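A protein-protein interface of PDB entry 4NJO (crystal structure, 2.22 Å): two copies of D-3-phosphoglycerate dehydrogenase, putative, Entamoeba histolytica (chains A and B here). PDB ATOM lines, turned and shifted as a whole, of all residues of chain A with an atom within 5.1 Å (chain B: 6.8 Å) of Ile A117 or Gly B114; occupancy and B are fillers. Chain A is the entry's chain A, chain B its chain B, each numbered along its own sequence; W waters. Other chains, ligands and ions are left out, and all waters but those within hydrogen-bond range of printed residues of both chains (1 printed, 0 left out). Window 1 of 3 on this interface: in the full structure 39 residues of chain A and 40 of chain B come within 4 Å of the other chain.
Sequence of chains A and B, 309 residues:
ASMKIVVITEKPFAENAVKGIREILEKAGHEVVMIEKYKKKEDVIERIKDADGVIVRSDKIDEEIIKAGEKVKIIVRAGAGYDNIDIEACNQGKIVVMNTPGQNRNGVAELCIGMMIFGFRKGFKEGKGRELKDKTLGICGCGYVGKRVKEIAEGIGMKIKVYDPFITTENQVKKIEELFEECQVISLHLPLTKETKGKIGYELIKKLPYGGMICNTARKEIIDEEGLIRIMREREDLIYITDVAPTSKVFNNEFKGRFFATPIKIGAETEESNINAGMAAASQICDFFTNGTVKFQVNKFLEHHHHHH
N of Leu A132 sits at hydrogen-bond distance from OE1 of Glu B110, 2.8 Å away.
Among the printed residues, pairs that only touch across the chains: Ile A117 with Glu B110 (3.4 Å), Phe A118 with Phe B118 (3.5 Å), Phe A124 with Leu B111 (3.6 Å), Ile A156 with Ile B152 (3.6 Å), Arg A121 with Leu B111 (3.7 Å), Ile A156 with Glu B110 (3.7 Å), Phe A124 with Phe B118 (3.7 Å), Gly A114 with Ile B117 (3.7 Å), Ile A117 with Gly B114 (3.7 Å), Phe A124 with Gly B114 (3.7 Å), Gly A114 with Phe B124 (3.8 Å), Phe A118 with Phe B124 (3.8 Å), Arg A121 with Glu B110 (3.9 Å), Phe A124 with Met B115 (3.97 Å), Ile A113 with Ile B117 (3.97 Å) and Met A115 with Phe B124 (3.98 Å).
Of chain A, only Ile A117 and Phe A124 come within 4 Å of Gly B114.
Of the printed residues of chain B, Phe A118 touches Phe B118 and Phe B124.
Printed residues of chain B within 4 Å of Leu A132: Glu B110.
Printed residues of chain A within 4 Å of Phe B124: Gly A114 (3.8 Å), Met A115 (3.98 Å) and Phe A118 (3.8 Å).
Met B116 touches none of the printed residues of chain A.
The nearest residue of chain B that does not touch Ile A117 is Ile B113 (4.2 Å).
The nearest residue of chain A that does not touch Gly B114 is Gly A114 (5.0 Å).
Hydrophobic or aromatic side chains of chain B within 4 Å of the printed part of chain A: Leu B111, Ile B117, Phe B118, Phe B124 and Ile B152.
Along chain B the printed residues that touch a printed residue of chain A span positions 110 to 152.
Printed residues of chain A that touch a printed residue of chain B: Ile A113, Gly A114, Met A115, Ile A117, Phe A118, Arg A121, Phe A124, Leu A132 and Ile A156.
Hydrophobic or aromatic side chains of chain A that line the printed part of chain B: Ile A113, Ile A117, Phe A118, Phe A124, Leu A132 and Ile A156.
Ile A113 touches Ile B117, but with the chains exchanged Ile A117 does not touch Ile B113 (4.2 Å).
Gly A114 touches Phe B124, and with the chains exchanged Phe A124 touches Gly B114.
Met A115 touches Phe B124, and with the chains exchanged Phe A124 touches Met B115.
Phe B118 touches its own counterpart, Phe A118.
8 positions are printed for both chains.
Of the 17 pairs that touch across the chains among the printed residues, 9 have their exchanged pair printed and touching as well.
Water W1 bridges the guanidinium group (NE) of Arg A121 (2.7 Å) and the side-chain carboxylate (OE1) of Glu B110 (2.8 Å).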
ATOM      1  N   ILE A 113      28.702   9.649  -0.338  1.00  0.00           N
ATOM      2  CA  ILE A 113      28.618   8.577  -1.340  1.00  0.00           C
ATOM      3  C   ILE A 113      27.352   8.704  -2.197  1.00  0.00           C
ATOM      4  O   ILE A 113      27.407   8.553  -3.421  1.00  0.00           O
ATOM      5  CB  ILE A 113      28.695   7.176  -0.677  1.00  0.00           C
ATOM      6  CG1 ILE A 113      30.087   6.934  -0.059  1.00  0.00           C
ATOM      7  CG2 ILE A 113      28.298   6.069  -1.655  1.00  0.00           C
ATOM      8  CD1 ILE A 113      31.206   6.651  -1.048  1.00  0.00           C
ATOM      9  N   GLY A 114      26.224   8.991  -1.553  1.00  0.00           N
ATOM     10  CA  GLY A 114      24.956   9.209  -2.256  1.00  0.00           C
ATOM     11  C   GLY A 114      25.011  10.389  -3.211  1.00  0.00           C
ATOM     12  O   GLY A 114      24.510  10.313  -4.338  1.00  0.00           O
ATOM     13  N   MET A 115      25.635  11.474  -2.756  1.00  0.00           N
ATOM     14  CA  MET A 115      25.825  12.685  -3.558  1.00  0.00           C
ATOM     15  C   MET A 115      26.731  12.460  -4.763  1.00  0.00           C
ATOM     16  O   MET A 115      26.516  13.048  -5.826  1.00  0.00           O
ATOM     17  CB  MET A 115      26.395  13.811  -2.696  1.00  0.00           C
ATOM     18  CG  MET A 115      25.357  14.528  -1.857  1.00  0.00           C
ATOM     19  SD  MET A 115      26.059  15.852  -0.856  1.00  0.00           S
ATOM     20  CE  MET A 115      24.598  16.871  -0.693  1.00  0.00           C
ATOM     21  N   MET A 116      27.744  11.613  -4.589  1.00  0.00           N
ATOM     22  CA  MET A 116      28.659  11.267  -5.676  1.00  0.00           C
ATOM     23  C   MET A 116      27.930  10.524  -6.788  1.00  0.00           C
ATOM     24  O   MET A 116      28.085  10.855  -7.966  1.00  0.00           O
ATOM     25  CB  MET A 116      29.834  10.434  -5.160  1.00  0.00           C
ATOM     26  CG  MET A 116      30.878  11.229  -4.394  1.00  0.00           C
ATOM     27  SD  MET A 116      32.105  10.157  -3.625  1.00  0.00           S
ATOM     28  CE  MET A 116      33.259  11.375  -3.025  1.00  0.00           C
ATOM     29  N   ILE A 117      27.130   9.528  -6.411  1.00  0.00           N
ATOM     30  CA  ILE A 117      26.323   8.783  -7.382  1.00  0.00           C
ATOM     31  C   ILE A 117      25.315   9.721  -8.049  1.00  0.00           C
ATOM     32  O   ILE A 117      25.248   9.792  -9.275  1.00  0.00           O
ATOM     33  CB  ILE A 117      25.622   7.561  -6.748  1.00  0.00           C
ATOM     34  CG1 ILE A 117      26.667   6.570  -6.212  1.00  0.00           C
ATOM     35  CG2 ILE A 117      24.719   6.879  -7.770  1.00  0.00           C
ATOM     36  CD1 ILE A 117      26.154   5.574  -5.188  1.00  0.00           C
ATOM     37  N   PHE A 118      24.560  10.452  -7.229  1.00  0.00           N
ATOM     38  CA  PHE A 118      23.604  11.457  -7.697  1.00  0.00           C
ATOM     39  C   PHE A 118      24.242  12.380  -8.741  1.00  0.00           C
ATOM     40  O   PHE A 118      23.695  12.566  -9.828  1.00  0.00           O
ATOM     41  CB  PHE A 118      23.083  12.260  -6.497  1.00  0.00           C
ATOM     42  CG  PHE A 118      21.937  13.184  -6.812  1.00  0.00           C
ATOM     43  CD1 PHE A 118      20.636  12.697  -6.913  1.00  0.00           C
ATOM     44  CD2 PHE A 118      22.152  14.549  -6.962  1.00  0.00           C
ATOM     45  CE1 PHE A 118      19.578  13.551  -7.184  1.00  0.00           C
ATOM     46  CE2 PHE A 118      21.096  15.408  -7.231  1.00  0.00           C
ATOM     47  CZ  PHE A 118      19.808  14.911  -7.340  1.00  0.00           C
ATOM     48  N   GLY A 119      25.414  12.924  -8.411  1.00  0.00           N
ATOM     49  CA  GLY A 119      26.138  13.836  -9.298  1.00  0.00           C
ATOM     50  C   GLY A 119      26.649  13.220 -10.590  1.00  0.00           C
ATOM     51  O   GLY A 119      26.604  13.856 -11.643  1.00  0.00           O
ATOM     52  N   PHE A 120      27.140  11.985 -10.511  1.00  0.00           N
ATOM     53  CA  PHE A 120      27.616  11.261 -11.692  1.00  0.00           C
ATOM     54  C   PHE A 120      26.472  10.750 -12.571  1.00  0.00           C
ATOM     55  O   PHE A 120      26.693  10.352 -13.715  1.00  0.00           O
ATOM     56  CB  PHE A 120      28.539  10.104 -11.279  1.00  0.00           C
ATOM     57  CG  PHE A 120      29.994  10.316 -11.628  1.00  0.00           C
ATOM     58  CD1 PHE A 120      30.540  11.596 -11.720  1.00  0.00           C
ATOM     59  CD2 PHE A 120      30.830   9.220 -11.849  1.00  0.00           C
ATOM     60  CE1 PHE A 120      31.880  11.779 -12.035  1.00  0.00           C
ATOM     61  CE2 PHE A 120      32.170   9.399 -12.166  1.00  0.00           C
ATOM     62  CZ  PHE A 120      32.695  10.681 -12.258  1.00  0.00           C
ATOM     63  N   ARG A 121      25.253  10.769 -12.037  1.00  0.00           N
ATOM     64  CA  ARG A 121      24.076  10.296 -12.766  1.00  0.00           C
ATOM     65  C   ARG A 121      23.067  11.402 -13.064  1.00  0.00           C
ATOM     66  O   ARG A 121      21.852  11.169 -13.025  1.00  0.00           O
ATOM     67  CB  ARG A 121      23.389   9.168 -11.999  1.00  0.00           C
ATOM     68  CG  ARG A 121      24.266   7.955 -11.765  1.00  0.00           C
ATOM     69  CD  ARG A 121      24.510   7.183 -13.047  1.00  0.00           C
ATOM     70  NE  ARG A 121      24.903   5.827 -12.708  1.00  0.00           N
ATOM     71  CZ  ARG A 121      24.182   4.743 -12.946  1.00  0.00           C
ATOM     72  NH1 ARG A 121      23.020   4.813 -13.581  1.00  0.00           N
ATOM     73  NH2 ARG A 121      24.658   3.577 -12.567  1.00  0.00           N
ATOM     74  N   PHE A 124      19.798  12.009 -11.191  1.00  0.00           N
ATOM     75  CA  PHE A 124      18.765  11.002 -11.486  1.00  0.00           C
ATOM     76  C   PHE A 124      17.803  11.403 -12.616  1.00  0.00           C
ATOM     77  O   PHE A 124      16.634  10.998 -12.631  1.00  0.00           O
ATOM     78  CB  PHE A 124      17.989  10.578 -10.223  1.00  0.00           C
ATOM     79  CG  PHE A 124      18.835   9.908  -9.167  1.00  0.00           C
ATOM     80  CD1 PHE A 124      20.054   9.310  -9.485  1.00  0.00           C
ATOM     81  CD2 PHE A 124      18.389   9.845  -7.848  1.00  0.00           C
ATOM     82  CE1 PHE A 124      20.821   8.694  -8.507  1.00  0.00           C
ATOM     83  CE2 PHE A 124      19.150   9.223  -6.867  1.00  0.00           C
ATOM     84  CZ  PHE A 124      20.367   8.647  -7.198  1.00  0.00           C
ATOM     85  N   LEU A 132      31.131   5.150 -10.804  1.00  0.00           N
ATOM     86  CA  LEU A 132      32.202   5.441  -9.851  1.00  0.00           C
ATOM     87  C   LEU A 132      33.272   4.352  -9.846  1.00  0.00           C
ATOM     88  O   LEU A 132      34.448   4.636  -9.616  1.00  0.00           O
ATOM     89  CB  LEU A 132      31.642   5.652  -8.437  1.00  0.00           C
ATOM     90  CG  LEU A 132      30.778   6.891  -8.159  1.00  0.00           C
ATOM     91  CD1 LEU A 132      30.184   6.815  -6.763  1.00  0.00           C
ATOM     92  CD2 LEU A 132      31.558   8.191  -8.326  1.00  0.00           C
ATOM     93  N   ILE A 156      32.766  -0.031  -3.747  1.00  0.00           N
ATOM     94  CA  ILE A 156      32.238   0.363  -5.058  1.00  0.00           C
ATOM     95  C   ILE A 156      33.268   0.085  -6.162  1.00  0.00           C
ATOM     96  O   ILE A 156      32.915  -0.068  -7.331  1.00  0.00           O
ATOM     97  CB  ILE A 156      31.790   1.851  -5.061  1.00  0.00           C
ATOM     98  CG1 ILE A 156      30.613   2.051  -4.095  1.00  0.00           C
ATOM     99  CG2 ILE A 156      31.410   2.321  -6.463  1.00  0.00           C
ATOM    100  CD1 ILE A 156      30.290   3.495  -3.767  1.00  0.00           C
ATOM    101  N   ALA B 109      23.434  -1.413 -10.404  1.00  0.00           N
ATOM    102  CA  ALA B 109      23.733  -1.564  -8.973  1.00  0.00           C
ATOM    103  C   ALA B 109      24.143  -0.252  -8.303  1.00  0.00           C
ATOM    104  O   ALA B 109      23.702   0.045  -7.190  1.00  0.00           O
ATOM    105  CB  ALA B 109      24.799  -2.632  -8.755  1.00  0.00           C
ATOM    106  N   GLU B 110      24.982   0.530  -8.981  1.00  0.00           N
ATOM    107  CA  GLU B 110      25.387   1.838  -8.462  1.00  0.00           C
ATOM    108  C   GLU B 110      24.190   2.781  -8.342  1.00  0.00           C
ATOM    109  O   GLU B 110      24.109   3.558  -7.390  1.00  0.00           O
ATOM    110  CB  GLU B 110      26.489   2.468  -9.319  1.00  0.00           C
ATOM    111  CG  GLU B 110      27.885   1.911  -9.056  1.00  0.00           C
ATOM    112  CD  GLU B 110      28.998   2.784  -9.625  1.00  0.00           C
ATOM    113  OE1 GLU B 110      28.786   4.004  -9.805  1.00  0.00           O
ATOM    114  OE2 GLU B 110      30.097   2.250  -9.886  1.00  0.00           O
ATOM    115  N   LEU B 111      23.264   2.702  -9.297  1.00  0.00           N
ATOM    116  CA  LEU B 111      22.040   3.504  -9.242  1.00  0.00           C
ATOM    117  C   LEU B 111      21.155   3.039  -8.095  1.00  0.00           C
ATOM    118  O   LEU B 111      20.576   3.856  -7.380  1.00  0.00           O
ATOM    119  CB  LEU B 111      21.267   3.453 -10.566  1.00  0.00           C
ATOM    120  CG  LEU B 111      19.973   4.284 -10.618  1.00  0.00           C
ATOM    121  CD1 LEU B 111      20.257   5.780 -10.616  1.00  0.00           C
ATOM    122  CD2 LEU B 111      19.133   3.910 -11.824  1.00  0.00           C
ATOM    123  N   CYS B 112      21.067   1.720  -7.925  1.00  0.00           N
ATOM    124  CA  CYS B 112      20.305   1.122  -6.839  1.00  0.00           C
ATOM    125  C   CYS B 112      20.795   1.595  -5.463  1.00  0.00           C
ATOM    126  O   CYS B 112      19.989   1.977  -4.613  1.00  0.00           O
ATOM    127  CB  CYS B 112      20.347  -0.405  -6.936  1.00  0.00           C
ATOM    128  SG  CYS B 112      19.374  -1.238  -5.668  1.00  0.00           S
ATOM    129  N   ILE B 113      22.108   1.575  -5.254  1.00  0.00           N
ATOM    130  CA  ILE B 113      22.702   2.065  -4.003  1.00  0.00           C
ATOM    131  C   ILE B 113      22.446   3.564  -3.816  1.00  0.00           C
ATOM    132  O   ILE B 113      22.064   4.002  -2.727  1.00  0.00           O
ATOM    133  CB  ILE B 113      24.218   1.767  -3.929  1.00  0.00           C
ATOM    134  CG1 ILE B 113      24.484   0.248  -3.967  1.00  0.00           C
ATOM    135  CG2 ILE B 113      24.848   2.417  -2.698  1.00  0.00           C
ATOM    136  CD1 ILE B 113      24.010  -0.529  -2.754  1.00  0.00           C
ATOM    137  N   GLY B 114      22.650   4.336  -4.882  1.00  0.00           N
ATOM    138  CA  GLY B 114      22.415   5.781  -4.856  1.00  0.00           C
ATOM    139  C   GLY B 114      20.980   6.130  -4.509  1.00  0.00           C
ATOM    140  O   GLY B 114      20.728   7.082  -3.773  1.00  0.00           O
ATOM    141  N   MET B 115      20.046   5.340  -5.033  1.00  0.00           N
ATOM    142  CA  MET B 115      18.620   5.522  -4.764  1.00  0.00           C
ATOM    143  C   MET B 115      18.254   5.166  -3.327  1.00  0.00           C
ATOM    144  O   MET B 115      17.373   5.794  -2.733  1.00  0.00           O
ATOM    145  CB  MET B 115      17.781   4.699  -5.740  1.00  0.00           C
ATOM    146  CG  MET B 115      17.638   5.335  -7.110  1.00  0.00           C
ATOM    147  SD  MET B 115      16.705   4.291  -8.240  1.00  0.00           S
ATOM    148  CE  MET B 115      16.433   5.443  -9.579  1.00  0.00           C
ATOM    149  N   MET B 116      18.935   4.164  -2.776  1.00  0.00           N
ATOM    150  CA  MET B 116      18.731   3.762  -1.386  1.00  0.00           C
ATOM    151  C   MET B 116      19.121   4.882  -0.416  1.00  0.00           C
ATOM    152  O   MET B 116      18.364   5.199   0.505  1.00  0.00           O
ATOM    153  CB  MET B 116      19.485   2.463  -1.075  1.00  0.00           C
ATOM    154  CG  MET B 116      18.798   1.206  -1.597  1.00  0.00           C
ATOM    155  SD  MET B 116      19.823  -0.282  -1.551  1.00  0.00           S
ATOM    156  CE  MET B 116      20.126  -0.429   0.205  1.00  0.00           C
ATOM    157  N   ILE B 117      20.287   5.487  -0.635  1.00  0.00           N
ATOM    158  CA  ILE B 117      20.739   6.620   0.183  1.00  0.00           C
ATOM    159  C   ILE B 117      19.811   7.824  -0.013  1.00  0.00           C
ATOM    160  O   ILE B 117      19.401   8.466   0.954  1.00  0.00           O
ATOM    161  CB  ILE B 117      22.209   7.003  -0.115  1.00  0.00           C
ATOM    162  CG1 ILE B 117      23.143   5.816   0.161  1.00  0.00           C
ATOM    163  CG2 ILE B 117      22.634   8.212   0.712  1.00  0.00           C
ATOM    164  CD1 ILE B 117      24.504   5.907  -0.508  1.00  0.00           C
ATOM    165  N   PHE B 118      19.470   8.099  -1.271  1.00  0.00           N
ATOM    166  CA  PHE B 118      18.581   9.198  -1.648  1.00  0.00           C
ATOM    167  C   PHE B 118      17.210   9.078  -0.978  1.00  0.00           C
ATOM    168  O   PHE B 118      16.667  10.067  -0.476  1.00  0.00           O
ATOM    169  CB  PHE B 118      18.430   9.218  -3.173  1.00  0.00           C
ATOM    170  CG  PHE B 118      17.703  10.419  -3.714  1.00  0.00           C
ATOM    171  CD1 PHE B 118      18.341  11.650  -3.816  1.00  0.00           C
ATOM    172  CD2 PHE B 118      16.391  10.310  -4.163  1.00  0.00           C
ATOM    173  CE1 PHE B 118      17.679  12.755  -4.335  1.00  0.00           C
ATOM    174  CE2 PHE B 118      15.722  11.411  -4.683  1.00  0.00           C
ATOM    175  CZ  PHE B 118      16.369  12.633  -4.773  1.00  0.00           C
ATOM    176  N   GLY B 119      16.668   7.862  -0.965  1.00  0.00           N
ATOM    177  CA  GLY B 119      15.360   7.592  -0.371  1.00  0.00           C
ATOM    178  C   GLY B 119      15.374   7.672   1.142  1.00  0.00           C
ATOM    179  O   GLY B 119      14.418   8.153   1.757  1.00  0.00           O
ATOM    180  N   PHE B 124      17.307  14.128  -0.390  1.00  0.00           N
ATOM    181  CA  PHE B 124      18.282  15.200  -0.139  1.00  0.00           C
ATOM    182  C   PHE B 124      17.630  16.540   0.226  1.00  0.00           C
ATOM    183  O   PHE B 124      18.179  17.607  -0.057  1.00  0.00           O
ATOM    184  CB  PHE B 124      19.276  15.362  -1.305  1.00  0.00           C
ATOM    185  CG  PHE B 124      20.126  14.144  -1.574  1.00  0.00           C
ATOM    186  CD1 PHE B 124      20.299  13.150  -0.609  1.00  0.00           C
ATOM    187  CD2 PHE B 124      20.788  14.009  -2.791  1.00  0.00           C
ATOM    188  CE1 PHE B 124      21.090  12.038  -0.865  1.00  0.00           C
ATOM    189  CE2 PHE B 124      21.585  12.900  -3.049  1.00  0.00           C
ATOM    190  CZ  PHE B 124      21.737  11.914  -2.085  1.00  0.00           C
ATOM    191  N   ILE B 152      28.302  -3.841  -2.454  1.00  0.00           N
ATOM    192  CA  ILE B 152      28.369  -2.438  -2.042  1.00  0.00           C
ATOM    193  C   ILE B 152      27.679  -2.247  -0.690  1.00  0.00           C
ATOM    194  O   ILE B 152      28.178  -1.517   0.171  1.00  0.00           O
ATOM    195  CB  ILE B 152      27.762  -1.492  -3.103  1.00  0.00           C
ATOM    196  CG1 ILE B 152      28.383  -1.762  -4.483  1.00  0.00           C
ATOM    197  CG2 ILE B 152      27.963  -0.035  -2.700  1.00  0.00           C
ATOM    198  CD1 ILE B 152      27.608  -1.184  -5.648  1.00  0.00           C
ATOM    199  N   ILE B 241      11.173   3.876  -4.146  1.00  0.00           N
ATOM    200  CA  ILE B 241      12.038   4.543  -5.111  1.00  0.00           C
ATOM    201  C   ILE B 241      12.301   3.596  -6.275  1.00  0.00           C
ATOM    202  O   ILE B 241      12.509   2.398  -6.072  1.00  0.00           O
ATOM    203  CB  ILE B 241      13.341   5.073  -4.456  1.00  0.00           C
ATOM    204  CG1 ILE B 241      14.151   5.909  -5.454  1.00  0.00           C
ATOM    205  CG2 ILE B 241      14.164   3.942  -3.842  1.00  0.00           C
ATOM    206  CD1 ILE B 241      14.985   6.991  -4.806  1.00  0.00           C
HETATM  207  O   HOH W   1      26.991   5.781 -10.968  1.00  0.00           O
